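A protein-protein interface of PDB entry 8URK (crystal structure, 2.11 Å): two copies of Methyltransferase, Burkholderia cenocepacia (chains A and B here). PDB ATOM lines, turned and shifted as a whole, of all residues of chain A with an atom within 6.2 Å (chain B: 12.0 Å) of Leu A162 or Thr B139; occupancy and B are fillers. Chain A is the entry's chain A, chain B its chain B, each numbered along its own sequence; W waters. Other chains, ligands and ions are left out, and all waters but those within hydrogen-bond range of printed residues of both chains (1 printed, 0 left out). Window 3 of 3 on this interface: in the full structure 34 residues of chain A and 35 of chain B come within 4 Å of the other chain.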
ATOM      1  N   PHE A 160     -13.889  -6.273  13.590  1.00  0.00           N
ATOM      2  CA  PHE A 160     -13.822  -7.691  13.896  1.00  0.00           C
ATOM      3  C   PHE A 160     -12.800  -8.362  12.998  1.00  0.00           C
ATOM      4  O   PHE A 160     -12.927  -8.304  11.792  1.00  0.00           O
ATOM      5  CB  PHE A 160     -15.198  -8.346  13.751  1.00  0.00           C
ATOM      6  CG  PHE A 160     -15.244  -9.783  14.170  1.00  0.00           C
ATOM      7  CD1 PHE A 160     -15.474 -10.125  15.486  1.00  0.00           C
ATOM      8  CD2 PHE A 160     -15.084 -10.790  13.241  1.00  0.00           C
ATOM      9  CE1 PHE A 160     -15.528 -11.443  15.875  1.00  0.00           C
ATOM     10  CE2 PHE A 160     -15.135 -12.116  13.624  1.00  0.00           C
ATOM     11  CZ  PHE A 160     -15.358 -12.440  14.943  1.00  0.00           C
ATOM     12  N   ASP A 161     -11.784  -8.968  13.589  1.00  0.00           N
ATOM     13  CA  ASP A 161     -10.763  -9.685  12.845  1.00  0.00           C
ATOM     14  C   ASP A 161     -10.739 -11.124  13.288  1.00  0.00           C
ATOM     15  O   ASP A 161     -10.314 -11.422  14.384  1.00  0.00           O
ATOM     16  CB  ASP A 161      -9.385  -9.045  13.029  1.00  0.00           C
ATOM     17  CG  ASP A 161      -8.289  -9.800  12.337  1.00  0.00           C
ATOM     18  OD1 ASP A 161      -8.559 -10.454  11.316  1.00  0.00           O
ATOM     19  OD2 ASP A 161      -7.148  -9.727  12.823  1.00  0.00           O
ATOM     20  N   LEU A 162     -11.158 -12.018  12.422  1.00  0.00           N
ATOM     21  CA  LEU A 162     -11.276 -13.416  12.806  1.00  0.00           C
ATOM     22  C   LEU A 162      -9.934 -14.126  12.836  1.00  0.00           C
ATOM     23  O   LEU A 162      -9.754 -15.078  13.610  1.00  0.00           O
ATOM     24  CB  LEU A 162     -12.210 -14.149  11.845  1.00  0.00           C
ATOM     25  CG  LEU A 162     -12.208 -15.654  12.061  1.00  0.00           C
ATOM     26  CD1 LEU A 162     -12.979 -15.939  13.333  1.00  0.00           C
ATOM     27  CD2 LEU A 162     -12.828 -16.338  10.880  1.00  0.00           C
ATOM     28  N   ASP A 163      -8.999 -13.711  11.990  1.00  0.00           N
ATOM     29  CA  ASP A 163      -7.765 -14.474  11.822  1.00  0.00           C
ATOM     30  C   ASP A 163      -7.061 -14.779  13.134  1.00  0.00           C
ATOM     31  O   ASP A 163      -6.709 -15.949  13.361  1.00  0.00           O
ATOM     32  CB  ASP A 163      -6.853 -13.727  10.842  1.00  0.00           C
ATOM     33  CG  ASP A 163      -7.305 -13.888   9.406  1.00  0.00           C
ATOM     34  OD1 ASP A 163      -8.393 -14.460   9.182  1.00  0.00           O
ATOM     35  OD2 ASP A 163      -6.563 -13.459   8.501  1.00  0.00           O
ATOM     36  N   PRO A 164      -6.845 -13.825  14.037  1.00  0.00           N
ATOM     37  CA  PRO A 164      -6.093 -14.142  15.257  1.00  0.00           C
ATOM     38  C   PRO A 164      -6.825 -15.084  16.201  1.00  0.00           C
ATOM     39  O   PRO A 164      -6.178 -15.657  17.087  1.00  0.00           O
ATOM     40  CB  PRO A 164      -5.859 -12.770  15.901  1.00  0.00           C
ATOM     41  CG  PRO A 164      -6.626 -11.769  15.070  1.00  0.00           C
ATOM     42  CD  PRO A 164      -7.482 -12.507  14.097  1.00  0.00           C
ATOM     43  N   VAL A 165      -8.140 -15.265  16.042  1.00  0.00           N
ATOM     44  CA  VAL A 165      -8.903 -16.173  16.888  1.00  0.00           C
ATOM     45  C   VAL A 165      -9.218 -17.493  16.200  1.00  0.00           C
ATOM     46  O   VAL A 165      -9.761 -18.398  16.851  1.00  0.00           O
ATOM     47  CB  VAL A 165     -10.207 -15.515  17.393  1.00  0.00           C
ATOM     48  CG1 VAL A 165      -9.900 -14.391  18.367  1.00  0.00           C
ATOM     49  CG2 VAL A 165     -11.074 -15.019  16.235  1.00  0.00           C
ATOM     50  N   ARG A 166      -8.886 -17.639  14.914  1.00  0.00           N
ATOM     51  CA  ARG A 166      -9.114 -18.904  14.219  1.00  0.00           C
ATOM     52  C   ARG A 166      -8.427 -20.054  14.946  1.00  0.00           C
ATOM     53  O   ARG A 166      -7.333 -19.900  15.495  1.00  0.00           O
ATOM     54  CB  ARG A 166      -8.606 -18.809  12.780  1.00  0.00           C
ATOM     55  CG  ARG A 166      -9.139 -17.591  12.033  1.00  0.00           C
ATOM     56  CD  ARG A 166      -8.690 -17.541  10.568  1.00  0.00           C
ATOM     57  NE  ARG A 166      -9.511 -18.412   9.739  1.00  0.00           N
ATOM     58  CZ  ARG A 166     -10.292 -18.011   8.744  1.00  0.00           C
ATOM     59  NH1 ARG A 166     -10.385 -16.735   8.403  1.00  0.00           N
ATOM     60  NH2 ARG A 166     -10.996 -18.917   8.070  1.00  0.00           N
ATOM     61  N   LYS A 186      -9.738 -21.180   3.616  1.00  0.00           N
ATOM     62  CA  LYS A 186      -9.093 -20.568   4.771  1.00  0.00           C
ATOM     63  C   LYS A 186      -9.443 -21.324   6.045  1.00  0.00           C
ATOM     64  O   LYS A 186      -8.560 -21.661   6.840  1.00  0.00           O
ATOM     65  CB  LYS A 186      -9.492 -19.100   4.886  1.00  0.00           C
ATOM     66  CG  LYS A 186      -8.761 -18.180   3.932  1.00  0.00           C
ATOM     67  CD  LYS A 186      -9.237 -16.746   4.084  1.00  0.00           C
ATOM     68  CE  LYS A 186      -8.383 -15.968   5.093  1.00  0.00           C
ATOM     69  NZ  LYS A 186      -7.571 -14.869   4.459  1.00  0.00           N
ATOM     70  N   GLY A 191      -7.503 -22.094   9.983  1.00  0.00           N
ATOM     71  CA  GLY A 191      -8.229 -22.528  11.160  1.00  0.00           C
ATOM     72  C   GLY A 191      -9.675 -22.124  11.015  1.00  0.00           C
ATOM     73  O   GLY A 191     -10.044 -21.338  10.148  1.00  0.00           O
ATOM     74  N   TYR A 192     -10.500 -22.673  11.903  1.00  0.00           N
ATOM     75  CA  TYR A 192     -11.932 -22.436  11.868  1.00  0.00           C
ATOM     76  C   TYR A 192     -12.488 -21.472  12.911  1.00  0.00           C
ATOM     77  O   TYR A 192     -11.861 -21.210  13.903  1.00  0.00           O
ATOM     78  CB  TYR A 192     -12.617 -23.794  12.021  1.00  0.00           C
ATOM     79  CG  TYR A 192     -12.324 -24.530  13.301  1.00  0.00           C
ATOM     80  CD1 TYR A 192     -13.107 -24.340  14.431  1.00  0.00           C
ATOM     81  CD2 TYR A 192     -11.288 -25.441  13.372  1.00  0.00           C
ATOM     82  CE1 TYR A 192     -12.848 -25.024  15.601  1.00  0.00           C
ATOM     83  CE2 TYR A 192     -11.018 -26.123  14.535  1.00  0.00           C
ATOM     84  CZ  TYR A 192     -11.802 -25.913  15.647  1.00  0.00           C
ATOM     85  OH  TYR A 192     -11.531 -26.596  16.803  1.00  0.00           O
ATOM     86  N   ASN A 193     -13.677 -20.965  12.671  1.00  0.00           N
ATOM     87  CA  ASN A 193     -14.335 -20.082  13.615  1.00  0.00           C
ATOM     88  C   ASN A 193     -14.600 -20.769  14.924  1.00  0.00           C
ATOM     89  O   ASN A 193     -14.963 -21.915  14.950  1.00  0.00           O
ATOM     90  CB  ASN A 193     -15.649 -19.618  13.018  1.00  0.00           C
ATOM     91  CG  ASN A 193     -16.286 -18.476  13.757  1.00  0.00           C
ATOM     92  OD1 ASN A 193     -16.460 -18.516  14.961  1.00  0.00           O
ATOM     93  ND2 ASN A 193     -16.684 -17.462  13.018  1.00  0.00           N
ATOM     94  N   PRO A 194     -14.394 -20.073  16.022  1.00  0.00           N
ATOM     95  CA  PRO A 194     -14.783 -20.681  17.295  1.00  0.00           C
ATOM     96  C   PRO A 194     -16.289 -21.008  17.405  1.00  0.00           C
ATOM     97  O   PRO A 194     -16.645 -21.709  18.317  1.00  0.00           O
ATOM     98  CB  PRO A 194     -14.426 -19.588  18.291  1.00  0.00           C
ATOM     99  CG  PRO A 194     -13.339 -18.809  17.643  1.00  0.00           C
ATOM    100  CD  PRO A 194     -13.697 -18.793  16.196  1.00  0.00           C
ATOM    101  N   ALA A 228     -10.262 -10.502  18.746  1.00  0.00           N
ATOM    102  CA  ALA A 228     -11.097 -10.438  17.581  1.00  0.00           C
ATOM    103  C   ALA A 228     -11.893  -9.167  17.448  1.00  0.00           C
ATOM    104  O   ALA A 228     -12.345  -8.835  16.371  1.00  0.00           O
ATOM    105  CB  ALA A 228     -12.027 -11.621  17.597  1.00  0.00           C
ATOM    106  N   PRO B 133     -21.706 -26.435  12.473  1.00  0.00           N
ATOM    107  CA  PRO B 133     -22.044 -25.022  12.317  1.00  0.00           C
ATOM    108  C   PRO B 133     -22.823 -24.696  11.071  1.00  0.00           C
ATOM    109  O   PRO B 133     -22.710 -25.405  10.095  1.00  0.00           O
ATOM    110  CB  PRO B 133     -20.668 -24.370  12.241  1.00  0.00           C
ATOM    111  CG  PRO B 133     -19.765 -25.415  11.728  1.00  0.00           C
ATOM    112  CD  PRO B 133     -20.269 -26.693  12.308  1.00  0.00           C
ATOM    113  N   SER B 134     -23.592 -23.640  11.110  1.00  0.00           N
ATOM    114  CA  SER B 134     -24.298 -23.184   9.927  1.00  0.00           C
ATOM    115  C   SER B 134     -23.295 -22.681   8.891  1.00  0.00           C
ATOM    116  O   SER B 134     -22.242 -22.197   9.240  1.00  0.00           O
ATOM    117  CB  SER B 134     -25.339 -22.097  10.235  1.00  0.00           C
ATOM    118  OG  SER B 134     -26.459 -22.573  10.922  1.00  0.00           O
ATOM    119  N   MET B 135     -23.631 -22.818   7.627  1.00  0.00           N
ATOM    120  CA  MET B 135     -22.762 -22.350   6.558  1.00  0.00           C
ATOM    121  C   MET B 135     -23.180 -20.972   6.035  1.00  0.00           C
ATOM    122  O   MET B 135     -24.253 -20.504   6.360  1.00  0.00           O
ATOM    123  CB  MET B 135     -22.732 -23.358   5.429  1.00  0.00           C
ATOM    124  CG  MET B 135     -22.194 -24.728   5.787  1.00  0.00           C
ATOM    125  SD  MET B 135     -20.403 -24.783   5.861  1.00  0.00           S
ATOM    126  CE  MET B 135     -20.136 -24.978   7.612  1.00  0.00           C
ATOM    127  N   GLY B 136     -22.335 -20.341   5.223  1.00  0.00           N
ATOM    128  CA  GLY B 136     -22.620 -19.037   4.648  1.00  0.00           C
ATOM    129  C   GLY B 136     -21.442 -18.391   3.925  1.00  0.00           C
ATOM    130  O   GLY B 136     -21.482 -18.188   2.737  1.00  0.00           O
ATOM    131  N   GLY B 137     -20.397 -18.073   4.651  1.00  0.00           N
ATOM    132  CA  GLY B 137     -19.259 -17.429   4.075  1.00  0.00           C
ATOM    133  C   GLY B 137     -18.693 -16.321   4.921  1.00  0.00           C
ATOM    134  O   GLY B 137     -17.683 -15.735   4.569  1.00  0.00           O
ATOM    135  N   THR B 138     -19.307 -16.054   6.052  1.00  0.00           N
ATOM    136  CA  THR B 138     -18.877 -14.944   6.868  1.00  0.00           C
ATOM    137  C   THR B 138     -17.578 -15.114   7.564  1.00  0.00           C
ATOM    138  O   THR B 138     -17.087 -16.196   7.707  1.00  0.00           O
ATOM    139  CB  THR B 138     -19.926 -14.538   7.939  1.00  0.00           C
ATOM    140  OG1 THR B 138     -19.637 -13.238   8.450  1.00  0.00           O
ATOM    141  CG2 THR B 138     -19.924 -15.533   9.082  1.00  0.00           C
ATOM    142  N   THR B 139     -17.027 -13.991   7.974  1.00  0.00           N
ATOM    143  CA  THR B 139     -15.794 -13.957   8.697  1.00  0.00           C
ATOM    144  C   THR B 139     -15.971 -12.777   9.638  1.00  0.00           C
ATOM    145  O   THR B 139     -15.095 -12.462  10.414  1.00  0.00           O
ATOM    146  CB  THR B 139     -14.617 -13.769   7.747  1.00  0.00           C
ATOM    147  OG1 THR B 139     -14.944 -12.758   6.791  1.00  0.00           O
ATOM    148  CG2 THR B 139     -14.307 -15.064   7.024  1.00  0.00           C
ATOM    149  N   ARG B 140     -17.141 -12.157   9.587  1.00  0.00           N
ATOM    150  CA  ARG B 140     -17.416 -10.984  10.413  1.00  0.00           C
ATOM    151  C   ARG B 140     -18.123 -11.239  11.762  1.00  0.00           C
ATOM    152  O   ARG B 140     -18.387 -10.311  12.500  1.00  0.00           O
ATOM    153  CB  ARG B 140     -18.191  -9.970   9.589  1.00  0.00           C
ATOM    154  CG  ARG B 140     -17.309  -8.998   8.835  1.00  0.00           C
ATOM    155  CD  ARG B 140     -18.094  -7.829   8.278  1.00  0.00           C
ATOM    156  NE  ARG B 140     -18.444  -6.833   9.286  1.00  0.00           N
ATOM    157  CZ  ARG B 140     -17.608  -6.329  10.187  1.00  0.00           C
ATOM    158  NH1 ARG B 140     -16.349  -6.716  10.238  1.00  0.00           N
ATOM    159  NH2 ARG B 140     -18.047  -5.433  11.045  1.00  0.00           N
ATOM    160  N   ARG B 141     -18.394 -12.496  12.085  1.00  0.00           N
ATOM    161  CA  ARG B 141     -19.011 -12.845  13.360  1.00  0.00           C
ATOM    162  C   ARG B 141     -18.757 -14.310  13.660  1.00  0.00           C
ATOM    163  O   ARG B 141     -18.128 -15.015  12.890  1.00  0.00           O
ATOM    164  CB  ARG B 141     -20.499 -12.554  13.372  1.00  0.00           C
ATOM    165  CG  ARG B 141     -21.354 -13.533  12.610  1.00  0.00           C
ATOM    166  CD  ARG B 141     -22.813 -13.207  12.816  1.00  0.00           C
ATOM    167  NE  ARG B 141     -23.351 -12.408  11.730  1.00  0.00           N
ATOM    168  CZ  ARG B 141     -24.206 -11.406  11.890  1.00  0.00           C
ATOM    169  NH1 ARG B 141     -24.626 -11.079  13.098  1.00  0.00           N
ATOM    170  NH2 ARG B 141     -24.643 -10.731  10.843  1.00  0.00           N
ATOM    171  N   PHE B 142     -19.260 -14.762  14.792  1.00  0.00           N
ATOM    172  CA  PHE B 142     -19.055 -16.132  15.147  1.00  0.00           C
ATOM    173  C   PHE B 142     -20.142 -16.980  14.510  1.00  0.00           C
ATOM    174  O   PHE B 142     -21.287 -16.635  14.534  1.00  0.00           O
ATOM    175  CB  PHE B 142     -18.928 -16.274  16.649  1.00  0.00           C
ATOM    176  CG  PHE B 142     -17.745 -15.579  17.237  1.00  0.00           C
ATOM    177  CD1 PHE B 142     -16.512 -16.195  17.269  1.00  0.00           C
ATOM    178  CD2 PHE B 142     -17.871 -14.319  17.780  1.00  0.00           C
ATOM    179  CE1 PHE B 142     -15.422 -15.559  17.819  1.00  0.00           C
ATOM    180  CE2 PHE B 142     -16.788 -13.676  18.333  1.00  0.00           C
ATOM    181  CZ  PHE B 142     -15.559 -14.296  18.351  1.00  0.00           C
ATOM    182  N   THR B 143     -19.737 -18.050  13.879  1.00  0.00           N
ATOM    183  CA  THR B 143     -20.652 -18.955  13.197  1.00  0.00           C
ATOM    184  C   THR B 143     -21.611 -19.648  14.158  1.00  0.00           C
ATOM    185  O   THR B 143     -21.288 -19.853  15.304  1.00  0.00           O
ATOM    186  CB  THR B 143     -19.831 -19.968  12.386  1.00  0.00           C
ATOM    187  OG1 THR B 143     -18.683 -20.368  13.129  1.00  0.00           O
ATOM    188  CG2 THR B 143     -19.391 -19.354  11.075  1.00  0.00           C
ATOM    189  N   SER B 144     -22.785 -20.003  13.685  1.00  0.00           N
ATOM    190  CA  SER B 144     -23.817 -20.563  14.548  1.00  0.00           C
ATOM    191  C   SER B 144     -23.806 -22.066  14.696  1.00  0.00           C
ATOM    192  O   SER B 144     -23.847 -22.770  13.722  1.00  0.00           O
ATOM    193  CB  SER B 144     -25.178 -20.084  14.069  1.00  0.00           C
ATOM    194  OG  SER B 144     -26.199 -21.038  14.265  1.00  0.00           O
HETATM  195  O   HOH W   1     -15.601 -17.315   9.704  1.00  0.00           O
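No position is printed for both chains.
The backbone NH (N) of Arg B140 is in hydrogen-bond range of the side-chain hydroxyl (OG1) of Thr B138.
Thr B139 touches Phe A160 (O to CE2, 3.2 Å).
Phe A160 touches Arg B140.
N of Arg B141 touches CE2 of Phe A160 (3.6 Å).
Phe B142 touches Phe A160 (CE2 to CE1, 3.6 Å).
Thr B139 touches Leu A162 (O to CB, 3.6 Å).
Phe B142 touches Asn A193 (CD1 to OD1, 3.3 Å).
Pro A194 touches Phe B142.
ND2 of Asn A193 sits at hydrogen-bond distance from O of Arg B141 (2.8 Å).
ND2 of Asn A193 lies close to N of Thr B143, 3.2 Å away.
Water W1 bridges the backbone carbonyl oxygen of Thr B138 (2.7 Å) and the side-chain amide nitrogen of Asn A193 (3.5 Å).
Along chain B the printed residues that touch a printed residue of chain A span positions 139 to 143.
Among the printed residues, 9 pairs touch across the chains.
Among the printed residues, no Asp or Glu carboxylate lies within 4 Å of a Lys or Arg side-chain nitrogen of the other chain.
Leu A162 touches just one residue of chain B: Thr B139 (3.6 Å).
Thr B139 touches just these residues of chain A: Phe A160 and Leu A162.
Phe A160 touches just these residues of chain B: Thr B139, Arg B140, Arg B141 and Phe B142.
No residue of chain B comes within 4 Å of Asp A161.
No residue of chain B comes within 4 Å of Asp A163.
No residue of chain B comes within 4 Å of Pro A164.
No residue of chain B comes within 4 Å of Val A165.
No residue of chain B comes within 4 Å of Arg A166.
No residue of chain B comes within 4 Å of Gly A191.
Asn A193 touches just these residues of chain B: Arg B141 (2.8 Å), Phe B142 (3.3 Å) and Thr B143 (3.1 Å).
Of the printed residues of chain A, Arg B140 touches Phe A160 (3.4 Å).
Of the printed residues of chain A, Arg B141 touches Phe A160 (3.6 Å) and Asn A193 (2.8 Å).
Printed residues of chain B within 4 Å of Pro A194: Phe B142 (3.9 Å).
Printed residues of chain A within 4 Å of Thr B143: Asn A193 (3.1 Å).
The nearest residue of chain B that does not touch Leu A162 is Phe B142 (5.1 Å).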
